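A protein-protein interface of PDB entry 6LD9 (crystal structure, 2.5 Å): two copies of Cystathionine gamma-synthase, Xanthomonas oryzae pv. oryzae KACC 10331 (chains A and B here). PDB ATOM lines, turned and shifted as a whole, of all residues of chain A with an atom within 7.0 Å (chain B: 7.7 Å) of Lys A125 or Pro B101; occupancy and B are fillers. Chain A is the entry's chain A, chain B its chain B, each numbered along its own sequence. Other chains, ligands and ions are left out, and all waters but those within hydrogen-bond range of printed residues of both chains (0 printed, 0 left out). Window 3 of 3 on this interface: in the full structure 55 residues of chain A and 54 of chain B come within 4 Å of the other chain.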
ATOM      1  N   PRO A 101      13.717  -8.207 -15.323  1.00  0.00           N
ATOM      2  CA  PRO A 101      12.479  -9.003 -15.392  1.00  0.00           C
ATOM      3  C   PRO A 101      11.323  -8.339 -14.643  1.00  0.00           C
ATOM      4  O   PRO A 101      11.569  -7.724 -13.560  1.00  0.00           O
ATOM      5  CB  PRO A 101      12.911 -10.287 -14.735  1.00  0.00           C
ATOM      6  CG  PRO A 101      14.379 -10.393 -15.178  1.00  0.00           C
ATOM      7  CD  PRO A 101      14.897  -9.001 -14.963  1.00  0.00           C
ATOM      8  N   ASN A 120      13.310  -9.942 -29.409  1.00  0.00           N
ATOM      9  CA  ASN A 120      12.443 -11.143 -29.423  1.00  0.00           C
ATOM     10  C   ASN A 120      13.206 -12.248 -28.690  1.00  0.00           C
ATOM     11  O   ASN A 120      12.603 -12.908 -27.858  1.00  0.00           O
ATOM     12  CB  ASN A 120      11.816 -11.370 -30.814  1.00  0.00           C
ATOM     13  CG  ASN A 120      10.683 -10.342 -31.107  1.00  0.00           C
ATOM     14  OD1 ASN A 120      10.882  -9.152 -31.568  1.00  0.00           O
ATOM     15  ND2 ASN A 120       9.449 -10.772 -30.815  1.00  0.00           N
ATOM     16  N   ALA A 121      14.521 -12.355 -28.834  1.00  0.00           N
ATOM     17  CA  ALA A 121      15.286 -13.419 -28.160  1.00  0.00           C
ATOM     18  C   ALA A 121      15.351 -13.144 -26.647  1.00  0.00           C
ATOM     19  O   ALA A 121      15.256 -14.097 -25.860  1.00  0.00           O
ATOM     20  CB  ALA A 121      16.650 -13.510 -28.770  1.00  0.00           C
ATOM     21  N   LEU A 122      15.560 -11.900 -26.224  1.00  0.00           N
ATOM     22  CA  LEU A 122      15.679 -11.598 -24.776  1.00  0.00           C
ATOM     23  C   LEU A 122      14.294 -11.647 -24.144  1.00  0.00           C
ATOM     24  O   LEU A 122      14.211 -12.061 -22.983  1.00  0.00           O
ATOM     25  CB  LEU A 122      16.343 -10.243 -24.533  1.00  0.00           C
ATOM     26  CG  LEU A 122      17.813 -10.125 -24.956  1.00  0.00           C
ATOM     27  CD1 LEU A 122      18.318  -8.711 -24.763  1.00  0.00           C
ATOM     28  CD2 LEU A 122      18.709 -11.072 -24.181  1.00  0.00           C
ATOM     29  N   ALA A 123      13.233 -11.326 -24.879  1.00  0.00           N
ATOM     30  CA  ALA A 123      11.820 -11.452 -24.406  1.00  0.00           C
ATOM     31  C   ALA A 123      11.471 -12.928 -24.237  1.00  0.00           C
ATOM     32  O   ALA A 123      10.942 -13.208 -23.182  1.00  0.00           O
ATOM     33  CB  ALA A 123      10.797 -10.779 -25.299  1.00  0.00           C
ATOM     34  N   LYS A 124      11.824 -13.821 -25.163  1.00  0.00           N
ATOM     35  CA  LYS A 124      11.532 -15.271 -25.032  1.00  0.00           C
ATOM     36  C   LYS A 124      12.196 -15.831 -23.766  1.00  0.00           C
ATOM     37  O   LYS A 124      11.579 -16.580 -23.097  1.00  0.00           O
ATOM     38  CB  LYS A 124      12.000 -16.061 -26.255  1.00  0.00           C
ATOM     39  CG  LYS A 124      11.098 -16.037 -27.505  1.00  0.00           C
ATOM     40  CD  LYS A 124      11.535 -17.076 -28.597  1.00  0.00           C
ATOM     41  CE  LYS A 124      12.006 -18.384 -27.945  1.00  0.00           C
ATOM     42  NZ  LYS A 124      12.550 -19.389 -28.889  1.00  0.00           N
ATOM     43  N   LYS A 125      13.415 -15.448 -23.442  1.00  0.00           N
ATOM     44  CA  LYS A 125      14.088 -15.821 -22.177  1.00  0.00           C
ATOM     45  C   LYS A 125      13.417 -15.176 -20.952  1.00  0.00           C
ATOM     46  O   LYS A 125      13.771 -15.551 -19.843  1.00  0.00           O
ATOM     47  CB  LYS A 125      15.529 -15.281 -22.130  1.00  0.00           C
ATOM     48  CG  LYS A 125      16.516 -15.767 -23.178  1.00  0.00           C
ATOM     49  CD  LYS A 125      17.958 -15.913 -22.681  1.00  0.00           C
ATOM     50  CE  LYS A 125      18.470 -17.211 -23.280  1.00  0.00           C
ATOM     51  NZ  LYS A 125      19.892 -17.435 -22.997  1.00  0.00           N
ATOM     52  N   GLY A 126      12.675 -14.085 -21.100  1.00  0.00           N
ATOM     53  CA  GLY A 126      12.013 -13.388 -19.973  1.00  0.00           C
ATOM     54  C   GLY A 126      12.866 -12.353 -19.252  1.00  0.00           C
ATOM     55  O   GLY A 126      12.622 -12.133 -18.062  1.00  0.00           O
ATOM     56  N   HIS A 127      13.751 -11.637 -19.944  1.00  0.00           N
ATOM     57  CA  HIS A 127      14.550 -10.526 -19.358  1.00  0.00           C
ATOM     58  C   HIS A 127      13.660  -9.308 -19.178  1.00  0.00           C
ATOM     59  O   HIS A 127      13.975  -8.451 -18.377  1.00  0.00           O
ATOM     60  CB  HIS A 127      15.744 -10.204 -20.261  1.00  0.00           C
ATOM     61  CG  HIS A 127      16.870 -11.164 -20.138  1.00  0.00           C
ATOM     62  ND1 HIS A 127      18.095 -10.914 -20.676  1.00  0.00           N
ATOM     63  CD2 HIS A 127      16.963 -12.354 -19.504  1.00  0.00           C
ATOM     64  CE1 HIS A 127      18.900 -11.931 -20.420  1.00  0.00           C
ATOM     65  NE2 HIS A 127      18.235 -12.811 -19.680  1.00  0.00           N
ATOM     66  N   PHE A 128      12.583  -9.232 -19.954  1.00  0.00           N
ATOM     67  CA  PHE A 128      11.553  -8.168 -19.863  1.00  0.00           C
ATOM     68  C   PHE A 128      10.369  -8.618 -20.705  1.00  0.00           C
ATOM     69  O   PHE A 128      10.511  -9.550 -21.511  1.00  0.00           O
ATOM     70  CB  PHE A 128      12.116  -6.821 -20.349  1.00  0.00           C
ATOM     71  CG  PHE A 128      12.887  -6.919 -21.640  1.00  0.00           C
ATOM     72  CD1 PHE A 128      12.231  -7.002 -22.856  1.00  0.00           C
ATOM     73  CD2 PHE A 128      14.278  -6.939 -21.643  1.00  0.00           C
ATOM     74  CE1 PHE A 128      12.958  -7.073 -24.050  1.00  0.00           C
ATOM     75  CE2 PHE A 128      14.999  -7.007 -22.837  1.00  0.00           C
ATOM     76  CZ  PHE A 128      14.337  -7.116 -24.032  1.00  0.00           C
ATOM     77  N   LEU B  93      28.985 -13.488 -23.145  1.00  0.00           N
ATOM     78  CA  LEU B  93      28.414 -14.274 -24.239  1.00  0.00           C
ATOM     79  C   LEU B  93      27.987 -15.631 -23.662  1.00  0.00           C
ATOM     80  O   LEU B  93      26.891 -16.052 -23.960  1.00  0.00           O
ATOM     81  CB  LEU B  93      29.453 -14.414 -25.345  1.00  0.00           C
ATOM     82  CG  LEU B  93      29.081 -15.381 -26.460  1.00  0.00           C
ATOM     83  CD1 LEU B  93      27.905 -14.846 -27.271  1.00  0.00           C
ATOM     84  CD2 LEU B  93      30.267 -15.643 -27.356  1.00  0.00           C
ATOM     85  N   VAL B  94      28.793 -16.269 -22.822  1.00  0.00           N
ATOM     86  CA  VAL B  94      28.491 -17.646 -22.359  1.00  0.00           C
ATOM     87  C   VAL B  94      27.247 -17.637 -21.458  1.00  0.00           C
ATOM     88  O   VAL B  94      26.388 -18.500 -21.698  1.00  0.00           O
ATOM     89  CB  VAL B  94      29.686 -18.286 -21.656  1.00  0.00           C
ATOM     90  CG1 VAL B  94      29.305 -19.574 -20.953  1.00  0.00           C
ATOM     91  CG2 VAL B  94      30.833 -18.520 -22.636  1.00  0.00           C
ATOM     92  N   LEU B  95      27.142 -16.719 -20.497  1.00  0.00           N
ATOM     93  CA  LEU B  95      25.930 -16.536 -19.651  1.00  0.00           C
ATOM     94  C   LEU B  95      24.673 -16.360 -20.530  1.00  0.00           C
ATOM     95  O   LEU B  95      23.700 -17.005 -20.279  1.00  0.00           O
ATOM     96  CB  LEU B  95      26.125 -15.320 -18.735  1.00  0.00           C
ATOM     97  CG  LEU B  95      27.343 -15.400 -17.828  1.00  0.00           C
ATOM     98  CD1 LEU B  95      27.371 -14.235 -16.861  1.00  0.00           C
ATOM     99  CD2 LEU B  95      27.433 -16.700 -17.079  1.00  0.00           C
ATOM    100  N   ASN B  96      24.697 -15.537 -21.568  1.00  0.00           N
ATOM    101  CA  ASN B  96      23.531 -15.283 -22.452  1.00  0.00           C
ATOM    102  C   ASN B  96      23.250 -16.516 -23.318  1.00  0.00           C
ATOM    103  O   ASN B  96      22.156 -16.779 -23.557  1.00  0.00           O
ATOM    104  CB  ASN B  96      23.751 -14.058 -23.340  1.00  0.00           C
ATOM    105  CG  ASN B  96      23.451 -12.784 -22.597  1.00  0.00           C
ATOM    106  OD1 ASN B  96      22.321 -12.296 -22.674  1.00  0.00           O
ATOM    107  ND2 ASN B  96      24.422 -12.283 -21.825  1.00  0.00           N
ATOM    108  N   ALA B  97      24.226 -17.234 -23.832  1.00  0.00           N
ATOM    109  CA  ALA B  97      23.923 -18.354 -24.725  1.00  0.00           C
ATOM    110  C   ALA B  97      23.413 -19.570 -23.937  1.00  0.00           C
ATOM    111  O   ALA B  97      22.828 -20.483 -24.511  1.00  0.00           O
ATOM    112  CB  ALA B  97      25.170 -18.710 -25.497  1.00  0.00           C
ATOM    113  N   VAL B  98      23.727 -19.658 -22.671  1.00  0.00           N
ATOM    114  CA  VAL B  98      23.585 -20.968 -21.991  1.00  0.00           C
ATOM    115  C   VAL B  98      22.482 -20.905 -20.936  1.00  0.00           C
ATOM    116  O   VAL B  98      21.932 -21.923 -20.726  1.00  0.00           O
ATOM    117  CB  VAL B  98      24.939 -21.399 -21.415  1.00  0.00           C
ATOM    118  CG1 VAL B  98      24.767 -22.513 -20.409  1.00  0.00           C
ATOM    119  CG2 VAL B  98      25.849 -21.831 -22.545  1.00  0.00           C
ATOM    120  N   LEU B  99      22.226 -19.754 -20.316  1.00  0.00           N
ATOM    121  CA  LEU B  99      21.391 -19.584 -19.100  1.00  0.00           C
ATOM    122  C   LEU B  99      20.138 -18.784 -19.456  1.00  0.00           C
ATOM    123  O   LEU B  99      20.238 -17.930 -20.324  1.00  0.00           O
ATOM    124  CB  LEU B  99      22.167 -18.824 -18.006  1.00  0.00           C
ATOM    125  CG  LEU B  99      23.387 -19.563 -17.457  1.00  0.00           C
ATOM    126  CD1 LEU B  99      24.165 -18.726 -16.419  1.00  0.00           C
ATOM    127  CD2 LEU B  99      22.962 -20.883 -16.861  1.00  0.00           C
ATOM    128  N   GLN B 100      19.013 -19.073 -18.795  1.00  0.00           N
ATOM    129  CA  GLN B 100      17.801 -18.221 -18.754  1.00  0.00           C
ATOM    130  C   GLN B 100      17.313 -18.216 -17.320  1.00  0.00           C
ATOM    131  O   GLN B 100      17.786 -19.018 -16.548  1.00  0.00           O
ATOM    132  CB  GLN B 100      16.736 -18.767 -19.700  1.00  0.00           C
ATOM    133  CG  GLN B 100      16.146 -20.090 -19.263  1.00  0.00           C
ATOM    134  CD  GLN B 100      15.353 -20.706 -20.389  1.00  0.00           C
ATOM    135  OE1 GLN B 100      15.265 -21.920 -20.503  1.00  0.00           O
ATOM    136  NE2 GLN B 100      14.786 -19.875 -21.249  1.00  0.00           N
ATOM    137  N   PRO B 101      16.410 -17.297 -16.906  1.00  0.00           N
ATOM    138  CA  PRO B 101      15.883 -17.273 -15.527  1.00  0.00           C
ATOM    139  C   PRO B 101      15.338 -18.621 -15.042  1.00  0.00           C
ATOM    140  O   PRO B 101      14.761 -19.342 -15.851  1.00  0.00           O
ATOM    141  CB  PRO B 101      14.778 -16.258 -15.665  1.00  0.00           C
ATOM    142  CG  PRO B 101      15.392 -15.276 -16.644  1.00  0.00           C
ATOM    143  CD  PRO B 101      15.913 -16.186 -17.725  1.00  0.00           C
ATOM    144  N   GLY B 102      15.667 -18.978 -13.802  1.00  0.00           N
ATOM    145  CA  GLY B 102      15.345 -20.287 -13.226  1.00  0.00           C
ATOM    146  C   GLY B 102      16.481 -21.286 -13.361  1.00  0.00           C
ATOM    147  O   GLY B 102      16.392 -22.327 -12.750  1.00  0.00           O
ATOM    148  N   ASP B 103      17.456 -21.049 -14.228  1.00  0.00           N
ATOM    149  CA  ASP B 103      18.672 -21.884 -14.330  1.00  0.00           C
ATOM    150  C   ASP B 103      19.609 -21.524 -13.169  1.00  0.00           C
ATOM    151  O   ASP B 103      19.630 -20.348 -12.726  1.00  0.00           O
ATOM    152  CB  ASP B 103      19.410 -21.630 -15.643  1.00  0.00           C
ATOM    153  CG  ASP B 103      18.807 -22.277 -16.864  1.00  0.00           C
ATOM    154  OD1 ASP B 103      17.929 -23.078 -16.625  1.00  0.00           O
ATOM    155  OD2 ASP B 103      19.279 -21.998 -18.047  1.00  0.00           O
ATOM    156  N   THR B 104      20.378 -22.467 -12.628  1.00  0.00           N
ATOM    157  CA  THR B 104      21.393 -22.010 -11.657  1.00  0.00           C
ATOM    158  C   THR B 104      22.788 -22.181 -12.264  1.00  0.00           C
ATOM    159  O   THR B 104      23.037 -23.139 -13.000  1.00  0.00           O
ATOM    160  CB  THR B 104      21.212 -22.498 -10.199  1.00  0.00           C
ATOM    161  OG1 THR B 104      22.171 -23.493  -9.908  1.00  0.00           O
ATOM    162  CG2 THR B 104      19.836 -22.975  -9.778  1.00  0.00           C
ATOM    163  N   LYS B 125      19.413  -8.950 -10.668  1.00  0.00           N
ATOM    164  CA  LYS B 125      18.303  -8.737 -11.613  1.00  0.00           C
ATOM    165  C   LYS B 125      17.470 -10.006 -11.858  1.00  0.00           C
ATOM    166  O   LYS B 125      16.437  -9.886 -12.477  1.00  0.00           O
ATOM    167  CB  LYS B 125      18.910  -8.398 -12.966  1.00  0.00           C
ATOM    168  CG  LYS B 125      19.588  -7.059 -13.115  1.00  0.00           C
ATOM    169  CD  LYS B 125      19.765  -6.854 -14.586  1.00  0.00           C
ATOM    170  CE  LYS B 125      19.672  -5.421 -15.009  1.00  0.00           C
ATOM    171  NZ  LYS B 125      19.976  -5.425 -16.450  1.00  0.00           N
ATOM    172  N   GLY B 126      17.978 -11.203 -11.574  1.00  0.00           N
ATOM    173  CA  GLY B 126      17.243 -12.477 -11.721  1.00  0.00           C
ATOM    174  C   GLY B 126      17.345 -13.095 -13.106  1.00  0.00           C
ATOM    175  O   GLY B 126      16.393 -13.753 -13.494  1.00  0.00           O
ATOM    176  N   HIS B 127      18.476 -12.969 -13.803  1.00  0.00           N
ATOM    177  CA  HIS B 127      18.769 -13.652 -15.089  1.00  0.00           C
ATOM    178  C   HIS B 127      19.061 -15.115 -14.819  1.00  0.00           C
ATOM    179  O   HIS B 127      18.884 -15.930 -15.699  1.00  0.00           O
ATOM    180  CB  HIS B 127      19.939 -12.970 -15.808  1.00  0.00           C
ATOM    181  CG  HIS B 127      19.587 -11.679 -16.456  1.00  0.00           C
ATOM    182  ND1 HIS B 127      20.439 -11.041 -17.315  1.00  0.00           N
ATOM    183  CD2 HIS B 127      18.459 -10.925 -16.403  1.00  0.00           C
ATOM    184  CE1 HIS B 127      19.883  -9.915 -17.732  1.00  0.00           C
ATOM    185  NE2 HIS B 127      18.649  -9.840 -17.223  1.00  0.00           N
ATOM    186  N   PHE B 128      19.587 -15.419 -13.641  1.00  0.00           N
ATOM    187  CA  PHE B 128      19.800 -16.809 -13.164  1.00  0.00           C
ATOM    188  C   PHE B 128      19.969 -16.758 -11.644  1.00  0.00           C
ATOM    189  O   PHE B 128      20.146 -15.680 -11.024  1.00  0.00           O
ATOM    190  CB  PHE B 128      21.011 -17.446 -13.862  1.00  0.00           C
ATOM    191  CG  PHE B 128      22.210 -16.531 -13.921  1.00  0.00           C
ATOM    192  CD1 PHE B 128      23.039 -16.370 -12.825  1.00  0.00           C
ATOM    193  CD2 PHE B 128      22.478 -15.792 -15.058  1.00  0.00           C
ATOM    194  CE1 PHE B 128      24.106 -15.467 -12.860  1.00  0.00           C
ATOM    195  CE2 PHE B 128      23.588 -14.955 -15.118  1.00  0.00           C
ATOM    196  CZ  PHE B 128      24.386 -14.769 -14.018  1.00  0.00           C
ATOM    197  N   ALA B 129      19.952 -17.919 -11.040  1.00  0.00           N
ATOM    198  CA  ALA B 129      20.271 -18.055  -9.607  1.00  0.00           C
ATOM    199  C   ALA B 129      21.758 -18.398  -9.497  1.00  0.00           C
ATOM    200  O   ALA B 129      22.296 -19.130 -10.336  1.00  0.00           O
ATOM    201  CB  ALA B 129      19.410 -19.136  -8.996  1.00  0.00           C
ATOM    202  N   TRP B 236      24.572 -15.838 -30.833  1.00  0.00           N
ATOM    203  CA  TRP B 236      24.393 -14.863 -29.733  1.00  0.00           C
ATOM    204  C   TRP B 236      25.430 -13.729 -29.856  1.00  0.00           C
ATOM    205  O   TRP B 236      25.103 -12.579 -29.509  1.00  0.00           O
ATOM    206  CB  TRP B 236      24.442 -15.569 -28.372  1.00  0.00           C
ATOM    207  CG  TRP B 236      23.147 -16.227 -28.018  1.00  0.00           C
ATOM    208  CD1 TRP B 236      22.858 -17.562 -28.089  1.00  0.00           C
ATOM    209  CD2 TRP B 236      21.954 -15.598 -27.527  1.00  0.00           C
ATOM    210  NE1 TRP B 236      21.562 -17.786 -27.753  1.00  0.00           N
ATOM    211  CE2 TRP B 236      20.980 -16.606 -27.406  1.00  0.00           C
ATOM    212  CE3 TRP B 236      21.614 -14.281 -27.221  1.00  0.00           C
ATOM    213  CZ2 TRP B 236      19.690 -16.362 -26.953  1.00  0.00           C
ATOM    214  CZ3 TRP B 236      20.334 -14.027 -26.790  1.00  0.00           C
ATOM    215  CH2 TRP B 236      19.398 -15.064 -26.618  1.00  0.00           C
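Printed residues of chain B within 4 Å of Pro A101: Lys B125 (3.1 Å). Printed residues of chain B within 4 Å of Ala A121: Trp B236. Printed residues of chain A within 4 Å of Pro B101: Lys A125. Of the printed residues of chain A, His B127 touches His A127 (3.5 Å). The nearest residue of chain A that does not touch Pro B101 is His A127 (4.4 Å). The nearest printed residue of chain A that does not touch Leu B99 is His A127 (5.5 Å).
Printed residues of chain A that touch a printed residue of chain B: Pro A101, Ala A121, Lys A125 and His A127. Hydrophobic or aromatic side chains of chain A that line the printed part of chain B: Pro A101, Ala A121 and His A127. Along chain A the printed residues that touch a printed residue of chain B span positions 101 to 127. Of the 18 printed residues of chain B, 6 touch a printed residue of chain A. Hydrophobic or aromatic side chains of chain B that line the printed part of chain A: Pro B101, His B127 and Trp B236. Among the printed residues, 7 pairs touch across the chains.
Pro A101 touches Lys B125, and with the chains exchanged Lys A125 touches Pro B101. His A127 touches its own counterpart, His B127.
The backbone carbonyl oxygen of Leu A122 lies within hydrogen-bond range of the backbone NH of His A127 (3.1 Å).
NZ of Lys A125 sits at hydrogen-bond distance from O of Asn B96, 2.4 Å away. NZ of Lys A125 is in hydrogen-bond range of O of Leu B99 (2.7 Å).
Lys B125 touches Pro A101 (O to CD, 3.1 Å). Ala A121 touches Trp B236 (CB to CH2, 3.8 Å). Lys A125 touches Pro B101 (O to CD, 3.1 Å). Lys A125 touches Trp B236. His B127 touches His A127 (CE1 to CE1, 3.5 Å).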
